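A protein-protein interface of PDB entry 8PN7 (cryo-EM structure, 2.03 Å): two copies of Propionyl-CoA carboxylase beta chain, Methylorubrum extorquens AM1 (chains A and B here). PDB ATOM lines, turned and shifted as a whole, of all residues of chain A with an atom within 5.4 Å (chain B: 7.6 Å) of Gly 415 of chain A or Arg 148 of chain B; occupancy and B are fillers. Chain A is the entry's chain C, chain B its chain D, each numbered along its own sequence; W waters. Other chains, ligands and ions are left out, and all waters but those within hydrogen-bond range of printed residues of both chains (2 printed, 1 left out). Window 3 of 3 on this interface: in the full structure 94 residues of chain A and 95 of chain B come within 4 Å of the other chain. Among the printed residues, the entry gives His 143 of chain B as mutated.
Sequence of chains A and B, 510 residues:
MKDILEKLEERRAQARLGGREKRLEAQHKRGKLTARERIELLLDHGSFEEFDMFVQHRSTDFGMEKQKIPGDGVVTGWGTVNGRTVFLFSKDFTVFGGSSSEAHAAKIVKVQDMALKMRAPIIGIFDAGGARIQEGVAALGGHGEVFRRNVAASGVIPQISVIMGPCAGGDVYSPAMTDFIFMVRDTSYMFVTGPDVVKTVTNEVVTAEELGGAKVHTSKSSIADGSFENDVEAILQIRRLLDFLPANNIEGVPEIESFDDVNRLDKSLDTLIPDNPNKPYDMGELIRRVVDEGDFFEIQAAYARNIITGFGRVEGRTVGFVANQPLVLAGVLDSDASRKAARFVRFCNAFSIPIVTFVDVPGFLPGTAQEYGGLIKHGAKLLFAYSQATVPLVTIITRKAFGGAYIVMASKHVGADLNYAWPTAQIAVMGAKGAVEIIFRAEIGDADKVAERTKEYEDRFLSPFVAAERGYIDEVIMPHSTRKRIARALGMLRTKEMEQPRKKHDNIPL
No position is printed for both chains.
Of the 7 pairs that touch across the chains among the printed residues, none has its exchanged pair printed and touching as well.
Printed residues of chain A that touch a printed residue of chain B: Ser 387, Lys 412, His 413 and Gly 415.
Hydrophobic or aromatic side chains of chain A that line the printed part of chain B: His 413.
Along chain A the printed residues that touch a printed residue of chain B span positions 387 to 415.
Hydrophobic or aromatic side chains of chain B that line the printed part of chain A: Val 151.
Among the printed residues, 7 pairs touch across the chains.
O of Lys 412 of chain A lies within hydrogen-bond range of NH2 of Arg 148 of chain B, 3.3 Å away.
NH2 of Arg 148 of chain B is in hydrogen-bond range of O of His 413 of chain A.
The backbone carbonyl oxygen (O) of His 413 of chain A sits close to the backbone carbonyl oxygen (O) of Gly 144 of chain B (3.3 Å).
Val 151 of chain B touches Ser 387 of chain A.
Gly 141 of chain B touches His 413 of chain A (CA to ND1, 3.3 Å).
His 413 of chain A touches Glu 145 of chain B.
CA of Gly 415 of chain A touches NH1 of Arg 148 of chain B (3.3 Å).
The side-chain carboxylate of Glu 145 of chain B is in salt-bridge range of the guanidinium group of Arg 148 of chain B (3.6 Å).
The backbone carbonyl oxygen (O) of Asp 417 of chain A lies within hydrogen-bond range of the side-chain amino group (NZ) of Lys 412 of chain A, 3.4 Å away.
The guanidinium group (NH1) of Arg 149 of chain B is in salt-bridge range of the side-chain carboxylate (OE1) of Glu 145 of chain B (3.1 Å).
Of the printed residues of chain A, Arg 148 of chain B touches Lys 412 (3.3 Å), His 413 (3.0 Å) and Gly 415 (3.3 Å).
Printed residues of chain A within 4 Å of Val 151 of chain B: Ser 387.
Printed residues of chain A within 4 Å of Gly 144 of chain B: His 413.
Printed residues of chain B within 4 Å of Ser 387 of chain A: Val 151 (3.6 Å).
Printed residues of chain A within 4 Å of Gly 141 of chain B: His 413 (3.3 Å).
The nearest residue of chain B that does not touch Gly 415 of chain A is Gly 144 of chain B (6.6 Å).
Water W1 lies within hydrogen-bond range of O of Ser 387 of chain A (3.0 Å) and O of Arg 148 of chain B (3.1 Å).
Water W2 lies within hydrogen-bond range of NH1 of Arg 148 of chain B (3.2 Å), O of Ser 387 of chain A (3.4 Å) and O of Val 414 of chain A (3.4 Å).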
ATOM      1  N   SER A 387     -27.457  17.240  -8.416  1.00  0.00           N
ATOM      2  CA  SER A 387     -27.200  16.149  -7.480  1.00  0.00           C
ATOM      3  C   SER A 387     -26.512  16.635  -6.210  1.00  0.00           C
ATOM      4  O   SER A 387     -26.636  16.001  -5.158  1.00  0.00           O
ATOM      5  CB  SER A 387     -26.356  15.070  -8.155  1.00  0.00           C
ATOM      6  OG  SER A 387     -26.953  14.634  -9.361  1.00  0.00           O
ATOM      7  N   ALA A 389     -27.120  19.581  -4.718  1.00  0.00           N
ATOM      8  CA  ALA A 389     -27.927  20.540  -3.975  1.00  0.00           C
ATOM      9  C   ALA A 389     -28.548  19.909  -2.733  1.00  0.00           C
ATOM     10  O   ALA A 389     -29.011  18.767  -2.758  1.00  0.00           O
ATOM     11  CB  ALA A 389     -29.023  21.113  -4.872  1.00  0.00           C
ATOM     12  N   LEU A 393     -35.889  21.040  -3.457  1.00  0.00           N
ATOM     13  CA  LEU A 393     -36.026  20.936  -4.904  1.00  0.00           C
ATOM     14  C   LEU A 393     -37.422  20.427  -5.221  1.00  0.00           C
ATOM     15  O   LEU A 393     -37.784  19.317  -4.820  1.00  0.00           O
ATOM     16  CB  LEU A 393     -34.967  20.004  -5.498  1.00  0.00           C
ATOM     17  CG  LEU A 393     -33.497  20.386  -5.313  1.00  0.00           C
ATOM     18  CD1 LEU A 393     -32.597  19.335  -5.937  1.00  0.00           C
ATOM     19  CD2 LEU A 393     -33.212  21.754  -5.907  1.00  0.00           C
ATOM     20  N   SER A 411     -34.547  15.285 -11.472  1.00  0.00           N
ATOM     21  CA  SER A 411     -35.400  14.131 -11.238  1.00  0.00           C
ATOM     22  C   SER A 411     -35.262  13.659  -9.789  1.00  0.00           C
ATOM     23  O   SER A 411     -34.366  14.072  -9.051  1.00  0.00           O
ATOM     24  CB  SER A 411     -35.051  12.998 -12.203  1.00  0.00           C
ATOM     25  OG  SER A 411     -33.720  12.556 -12.009  1.00  0.00           O
ATOM     26  N   LYS A 412     -36.179  12.780  -9.382  1.00  0.00           N
ATOM     27  CA  LYS A 412     -36.117  12.228  -8.033  1.00  0.00           C
ATOM     28  C   LYS A 412     -34.847  11.415  -7.820  1.00  0.00           C
ATOM     29  O   LYS A 412     -34.339  11.338  -6.696  1.00  0.00           O
ATOM     30  CB  LYS A 412     -37.354  11.372  -7.758  1.00  0.00           C
ATOM     31  CG  LYS A 412     -37.436  10.836  -6.337  1.00  0.00           C
ATOM     32  CD  LYS A 412     -38.801  10.242  -6.042  1.00  0.00           C
ATOM     33  CE  LYS A 412     -39.900  11.284  -6.180  1.00  0.00           C
ATOM     34  NZ  LYS A 412     -39.694  12.443  -5.267  1.00  0.00           N
ATOM     35  N   HIS A 413     -34.313  10.820  -8.887  1.00  0.00           N
ATOM     36  CA  HIS A 413     -33.134   9.972  -8.770  1.00  0.00           C
ATOM     37  C   HIS A 413     -31.874  10.756  -8.425  1.00  0.00           C
ATOM     38  O   HIS A 413     -30.931  10.173  -7.884  1.00  0.00           O
ATOM     39  CB  HIS A 413     -32.929   9.197 -10.071  1.00  0.00           C
ATOM     40  CG  HIS A 413     -34.208   8.808 -10.742  1.00  0.00           C
ATOM     41  ND1 HIS A 413     -35.071   7.874 -10.214  1.00  0.00           N
ATOM     42  CD2 HIS A 413     -34.776   9.237 -11.893  1.00  0.00           C
ATOM     43  CE1 HIS A 413     -36.114   7.740 -11.012  1.00  0.00           C
ATOM     44  NE2 HIS A 413     -35.960   8.556 -12.039  1.00  0.00           N
ATOM     45  N   VAL A 414     -31.829  12.057  -8.725  1.00  0.00           N
ATOM     46  CA  VAL A 414     -30.670  12.875  -8.387  1.00  0.00           C
ATOM     47  C   VAL A 414     -30.866  13.658  -7.097  1.00  0.00           C
ATOM     48  O   VAL A 414     -29.972  14.417  -6.703  1.00  0.00           O
ATOM     49  CB  VAL A 414     -30.296  13.832  -9.538  1.00  0.00           C
ATOM     50  CG1 VAL A 414     -30.063  13.052 -10.822  1.00  0.00           C
ATOM     51  CG2 VAL A 414     -31.362  14.891  -9.733  1.00  0.00           C
ATOM     52  N   GLY A 415     -32.005  13.499  -6.428  1.00  0.00           N
ATOM     53  CA  GLY A 415     -32.188  14.098  -5.121  1.00  0.00           C
ATOM     54  C   GLY A 415     -33.304  15.116  -5.004  1.00  0.00           C
ATOM     55  O   GLY A 415     -33.356  15.861  -4.024  1.00  0.00           O
ATOM     56  N   ALA A 416     -34.197  15.169  -5.988  1.00  0.00           N
ATOM     57  CA  ALA A 416     -35.347  16.057  -5.889  1.00  0.00           C
ATOM     58  C   ALA A 416     -36.259  15.612  -4.751  1.00  0.00           C
ATOM     59  O   ALA A 416     -36.439  14.417  -4.507  1.00  0.00           O
ATOM     60  CB  ALA A 416     -36.118  16.086  -7.207  1.00  0.00           C
ATOM     61  N   ASP A 417     -36.832  16.588  -4.047  1.00  0.00           N
ATOM     62  CA  ASP A 417     -37.660  16.283  -2.885  1.00  0.00           C
ATOM     63  C   ASP A 417     -39.071  15.882  -3.292  1.00  0.00           C
ATOM     64  O   ASP A 417     -39.571  14.832  -2.878  1.00  0.00           O
ATOM     65  CB  ASP A 417     -37.690  17.484  -1.941  1.00  0.00           C
ATOM     66  CG  ASP A 417     -36.332  17.790  -1.355  1.00  0.00           C
ATOM     67  OD1 ASP A 417     -35.763  16.905  -0.683  1.00  0.00           O
ATOM     68  OD2 ASP A 417     -35.822  18.905  -1.584  1.00  0.00           O
ATOM     69  N   LYS A 496     -35.904  21.346   5.627  1.00  0.00           N
ATOM     70  CA  LYS A 496     -35.064  20.284   5.087  1.00  0.00           C
ATOM     71  C   LYS A 496     -33.639  20.393   5.616  1.00  0.00           C
ATOM     72  O   LYS A 496     -33.056  21.479   5.660  1.00  0.00           O
ATOM     73  CB  LYS A 496     -35.066  20.341   3.559  1.00  0.00           C
ATOM     74  CG  LYS A 496     -34.156  19.328   2.890  1.00  0.00           C
ATOM     75  CD  LYS A 496     -34.125  19.536   1.387  1.00  0.00           C
ATOM     76  CE  LYS A 496     -33.232  18.519   0.706  1.00  0.00           C
ATOM     77  NZ  LYS A 496     -33.134  18.767  -0.755  1.00  0.00           N
ATOM     78  N   VAL B 109     -24.341   0.732  -7.973  1.00  0.00           N
ATOM     79  CA  VAL B 109     -24.609   1.543  -6.789  1.00  0.00           C
ATOM     80  C   VAL B 109     -24.025   0.886  -5.544  1.00  0.00           C
ATOM     81  O   VAL B 109     -23.471   1.565  -4.672  1.00  0.00           O
ATOM     82  CB  VAL B 109     -26.124   1.789  -6.651  1.00  0.00           C
ATOM     83  CG1 VAL B 109     -26.499   2.077  -5.209  1.00  0.00           C
ATOM     84  CG2 VAL B 109     -26.553   2.934  -7.551  1.00  0.00           C
ATOM     85  N   GLN B 112     -20.315   1.477  -5.610  1.00  0.00           N
ATOM     86  CA  GLN B 112     -20.032   2.879  -5.306  1.00  0.00           C
ATOM     87  C   GLN B 112     -20.179   3.169  -3.817  1.00  0.00           C
ATOM     88  O   GLN B 112     -19.340   3.859  -3.223  1.00  0.00           O
ATOM     89  CB  GLN B 112     -20.957   3.790  -6.112  1.00  0.00           C
ATOM     90  CG  GLN B 112     -20.661   3.844  -7.594  1.00  0.00           C
ATOM     91  CD  GLN B 112     -21.653   4.706  -8.343  1.00  0.00           C
ATOM     92  OE1 GLN B 112     -22.824   4.353  -8.469  1.00  0.00           O
ATOM     93  NE2 GLN B 112     -21.193   5.848  -8.835  1.00  0.00           N
ATOM     94  N   LEU B 116     -17.220   4.399  -1.280  1.00  0.00           N
ATOM     95  CA  LEU B 116     -17.306   5.634  -0.509  1.00  0.00           C
ATOM     96  C   LEU B 116     -17.190   5.365   0.988  1.00  0.00           C
ATOM     97  O   LEU B 116     -16.515   6.111   1.704  1.00  0.00           O
ATOM     98  CB  LEU B 116     -18.607   6.368  -0.826  1.00  0.00           C
ATOM     99  CG  LEU B 116     -18.786   7.700  -0.096  1.00  0.00           C
ATOM    100  CD1 LEU B 116     -17.618   8.630  -0.377  1.00  0.00           C
ATOM    101  CD2 LEU B 116     -20.097   8.362  -0.481  1.00  0.00           C
ATOM    102  N   GLY B 141     -33.808   5.620 -13.873  1.00  0.00           N
ATOM    103  CA  GLY B 141     -33.698   5.791 -12.434  1.00  0.00           C
ATOM    104  C   GLY B 141     -32.406   5.227 -11.875  1.00  0.00           C
ATOM    105  O   GLY B 141     -31.768   5.836 -11.009  1.00  0.00           O
ATOM    106  N   GLY B 142     -32.003   4.052 -12.361  1.00  0.00           N
ATOM    107  CA  GLY B 142     -30.728   3.493 -11.938  1.00  0.00           C
ATOM    108  C   GLY B 142     -29.548   4.357 -12.342  1.00  0.00           C
ATOM    109  O   GLY B 142     -28.609   4.555 -11.563  1.00  0.00           O
ATOM    110  N   HIS B 143     -29.579   4.878 -13.571  1.00  0.00           N
ATOM    111  CA  HIS B 143     -28.551   5.818 -14.006  1.00  0.00           C
ATOM    112  C   HIS B 143     -28.502   7.039 -13.097  1.00  0.00           C
ATOM    113  O   HIS B 143     -27.419   7.525 -12.758  1.00  0.00           O
ATOM    114  CB  HIS B 143     -28.803   6.242 -15.450  1.00  0.00           C
ATOM    115  CG  HIS B 143     -28.047   5.436 -16.459  1.00  0.00           C
ATOM    116  ND1 HIS B 143     -28.492   5.258 -17.750  1.00  0.00           N
ATOM    117  CD2 HIS B 143     -26.872   4.771 -16.369  1.00  0.00           C
ATOM    118  CE1 HIS B 143     -27.626   4.511 -18.412  1.00  0.00           C
ATOM    119  NE2 HIS B 143     -26.634   4.204 -17.596  1.00  0.00           N
ATOM    120  N   GLY B 144     -29.668   7.553 -12.707  1.00  0.00           N
ATOM    121  CA  GLY B 144     -29.701   8.696 -11.808  1.00  0.00           C
ATOM    122  C   GLY B 144     -29.104   8.389 -10.448  1.00  0.00           C
ATOM    123  O   GLY B 144     -28.415   9.225  -9.860  1.00  0.00           O
ATOM    124  N   GLU B 145     -29.370   7.190  -9.925  1.00  0.00           N
ATOM    125  CA  GLU B 145     -28.750   6.787  -8.663  1.00  0.00           C
ATOM    126  C   GLU B 145     -27.231   6.729  -8.790  1.00  0.00           C
ATOM    127  O   GLU B 145     -26.499   7.188  -7.898  1.00  0.00           O
ATOM    128  CB  GLU B 145     -29.304   5.436  -8.210  1.00  0.00           C
ATOM    129  CG  GLU B 145     -30.804   5.421  -7.971  1.00  0.00           C
ATOM    130  CD  GLU B 145     -31.234   6.373  -6.873  1.00  0.00           C
ATOM    131  OE1 GLU B 145     -30.456   6.580  -5.921  1.00  0.00           O
ATOM    132  OE2 GLU B 145     -32.354   6.919  -6.965  1.00  0.00           O
ATOM    133  N   VAL B 146     -26.740   6.177  -9.903  1.00  0.00           N
ATOM    134  CA  VAL B 146     -25.298   6.135 -10.139  1.00  0.00           C
ATOM    135  C   VAL B 146     -24.723   7.547 -10.209  1.00  0.00           C
ATOM    136  O   VAL B 146     -23.653   7.824  -9.655  1.00  0.00           O
ATOM    137  CB  VAL B 146     -24.984   5.330 -11.415  1.00  0.00           C
ATOM    138  CG1 VAL B 146     -23.499   5.375 -11.723  1.00  0.00           C
ATOM    139  CG2 VAL B 146     -25.451   3.892 -11.263  1.00  0.00           C
ATOM    140  N   PHE B 147     -25.419   8.458 -10.896  1.00  0.00           N
ATOM    141  CA  PHE B 147     -24.954   9.840 -10.996  1.00  0.00           C
ATOM    142  C   PHE B 147     -24.903  10.508  -9.628  1.00  0.00           C
ATOM    143  O   PHE B 147     -23.958  11.246  -9.318  1.00  0.00           O
ATOM    144  CB  PHE B 147     -25.865  10.640 -11.928  1.00  0.00           C
ATOM    145  CG  PHE B 147     -25.929  10.111 -13.325  1.00  0.00           C
ATOM    146  CD1 PHE B 147     -24.873   9.398 -13.863  1.00  0.00           C
ATOM    147  CD2 PHE B 147     -27.050  10.330 -14.107  1.00  0.00           C
ATOM    148  CE1 PHE B 147     -24.936   8.913 -15.150  1.00  0.00           C
ATOM    149  CE2 PHE B 147     -27.117   9.848 -15.394  1.00  0.00           C
ATOM    150  CZ  PHE B 147     -26.060   9.139 -15.916  1.00  0.00           C
ATOM    151  N   ARG B 148     -25.931  10.280  -8.810  1.00  0.00           N
ATOM    152  CA  ARG B 148     -25.959  10.853  -7.472  1.00  0.00           C
ATOM    153  C   ARG B 148     -24.775  10.369  -6.648  1.00  0.00           C
ATOM    154  O   ARG B 148     -24.141  11.154  -5.934  1.00  0.00           O
ATOM    155  CB  ARG B 148     -27.278  10.501  -6.783  1.00  0.00           C
ATOM    156  CG  ARG B 148     -27.496  11.198  -5.458  1.00  0.00           C
ATOM    157  CD  ARG B 148     -28.212  10.288  -4.475  1.00  0.00           C
ATOM    158  NE  ARG B 148     -29.531   9.885  -4.944  1.00  0.00           N
ATOM    159  CZ  ARG B 148     -30.666  10.457  -4.567  1.00  0.00           C
ATOM    160  NH1 ARG B 148     -30.679  11.466  -3.712  1.00  0.00           N
ATOM    161  NH2 ARG B 148     -31.816   9.998  -5.053  1.00  0.00           N
ATOM    162  N   ARG B 149     -24.445   9.080  -6.751  1.00  0.00           N
ATOM    163  CA  ARG B 149     -23.292   8.587  -6.002  1.00  0.00           C
ATOM    164  C   ARG B 149     -21.972   9.097  -6.576  1.00  0.00           C
ATOM    165  O   ARG B 149     -21.023   9.332  -5.818  1.00  0.00           O
ATOM    166  CB  ARG B 149     -23.322   7.065  -5.938  1.00  0.00           C
ATOM    167  CG  ARG B 149     -24.126   6.576  -4.754  1.00  0.00           C
ATOM    168  CD  ARG B 149     -24.888   5.316  -5.057  1.00  0.00           C
ATOM    169  NE  ARG B 149     -25.824   5.006  -3.984  1.00  0.00           N
ATOM    170  CZ  ARG B 149     -27.078   5.434  -3.939  1.00  0.00           C
ATOM    171  NH1 ARG B 149     -27.585   6.191  -4.898  1.00  0.00           N
ATOM    172  NH2 ARG B 149     -27.843   5.090  -2.908  1.00  0.00           N
ATOM    173  N   ASN B 150     -21.893   9.287  -7.895  1.00  0.00           N
ATOM    174  CA  ASN B 150     -20.713   9.918  -8.483  1.00  0.00           C
ATOM    175  C   ASN B 150     -20.499  11.314  -7.916  1.00  0.00           C
ATOM    176  O   ASN B 150     -19.369  11.697  -7.593  1.00  0.00           O
ATOM    177  CB  ASN B 150     -20.844   9.991 -10.005  1.00  0.00           C
ATOM    178  CG  ASN B 150     -20.447   8.705 -10.695  1.00  0.00           C
ATOM    179  OD1 ASN B 150     -21.166   8.204 -11.555  1.00  0.00           O
ATOM    180  ND2 ASN B 150     -19.293   8.168 -10.327  1.00  0.00           N
ATOM    181  N   VAL B 151     -21.577  12.092  -7.801  1.00  0.00           N
ATOM    182  CA  VAL B 151     -21.461  13.446  -7.268  1.00  0.00           C
ATOM    183  C   VAL B 151     -21.115  13.414  -5.785  1.00  0.00           C
ATOM    184  O   VAL B 151     -20.324  14.231  -5.300  1.00  0.00           O
ATOM    185  CB  VAL B 151     -22.753  14.239  -7.538  1.00  0.00           C
ATOM    186  CG1 VAL B 151     -22.740  15.561  -6.786  1.00  0.00           C
ATOM    187  CG2 VAL B 151     -22.912  14.480  -9.026  1.00  0.00           C
ATOM    188  N   ALA B 152     -21.696  12.470  -5.041  1.00  0.00           N
ATOM    189  CA  ALA B 152     -21.392  12.365  -3.617  1.00  0.00           C
ATOM    190  C   ALA B 152     -19.925  12.018  -3.388  1.00  0.00           C
ATOM    191  O   ALA B 152     -19.300  12.527  -2.451  1.00  0.00           O
ATOM    192  CB  ALA B 152     -22.301  11.329  -2.959  1.00  0.00           C
ATOM    193  N   ALA B 153     -19.358  11.159  -4.234  1.00  0.00           N
ATOM    194  CA  ALA B 153     -17.972  10.740  -4.064  1.00  0.00           C
ATOM    195  C   ALA B 153     -16.962  11.747  -4.601  1.00  0.00           C
ATOM    196  O   ALA B 153     -15.759  11.546  -4.413  1.00  0.00           O
ATOM    197  CB  ALA B 153     -17.744   9.386  -4.741  1.00  0.00           C
ATOM    198  N   SER B 154     -17.412  12.816  -5.254  1.00  0.00           N
ATOM    199  CA  SER B 154     -16.494  13.754  -5.892  1.00  0.00           C
ATOM    200  C   SER B 154     -15.693  14.523  -4.849  1.00  0.00           C
ATOM    201  O   SER B 154     -16.259  15.150  -3.949  1.00  0.00           O
ATOM    202  CB  SER B 154     -17.267  14.719  -6.787  1.00  0.00           C
ATOM    203  OG  SER B 154     -16.392  15.603  -7.460  1.00  0.00           O
ATOM    204  N   MET B 177     -18.380  12.982 -14.736  1.00  0.00           N
ATOM    205  CA  MET B 177     -18.265  13.524 -13.393  1.00  0.00           C
ATOM    206  C   MET B 177     -17.134  12.889 -12.595  1.00  0.00           C
ATOM    207  O   MET B 177     -16.894  13.300 -11.456  1.00  0.00           O
ATOM    208  CB  MET B 177     -19.597  13.369 -12.653  1.00  0.00           C
ATOM    209  CG  MET B 177     -20.733  14.152 -13.303  1.00  0.00           C
ATOM    210  SD  MET B 177     -22.331  13.931 -12.507  1.00  0.00           S
ATOM    211  CE  MET B 177     -22.519  12.157 -12.635  1.00  0.00           C
HETATM  212  O   HOH W   1     -24.998  13.666  -4.320  1.00  0.00           O
HETATM  213  O   HOH W   2     -28.866  14.036  -3.463  1.00  0.00           O
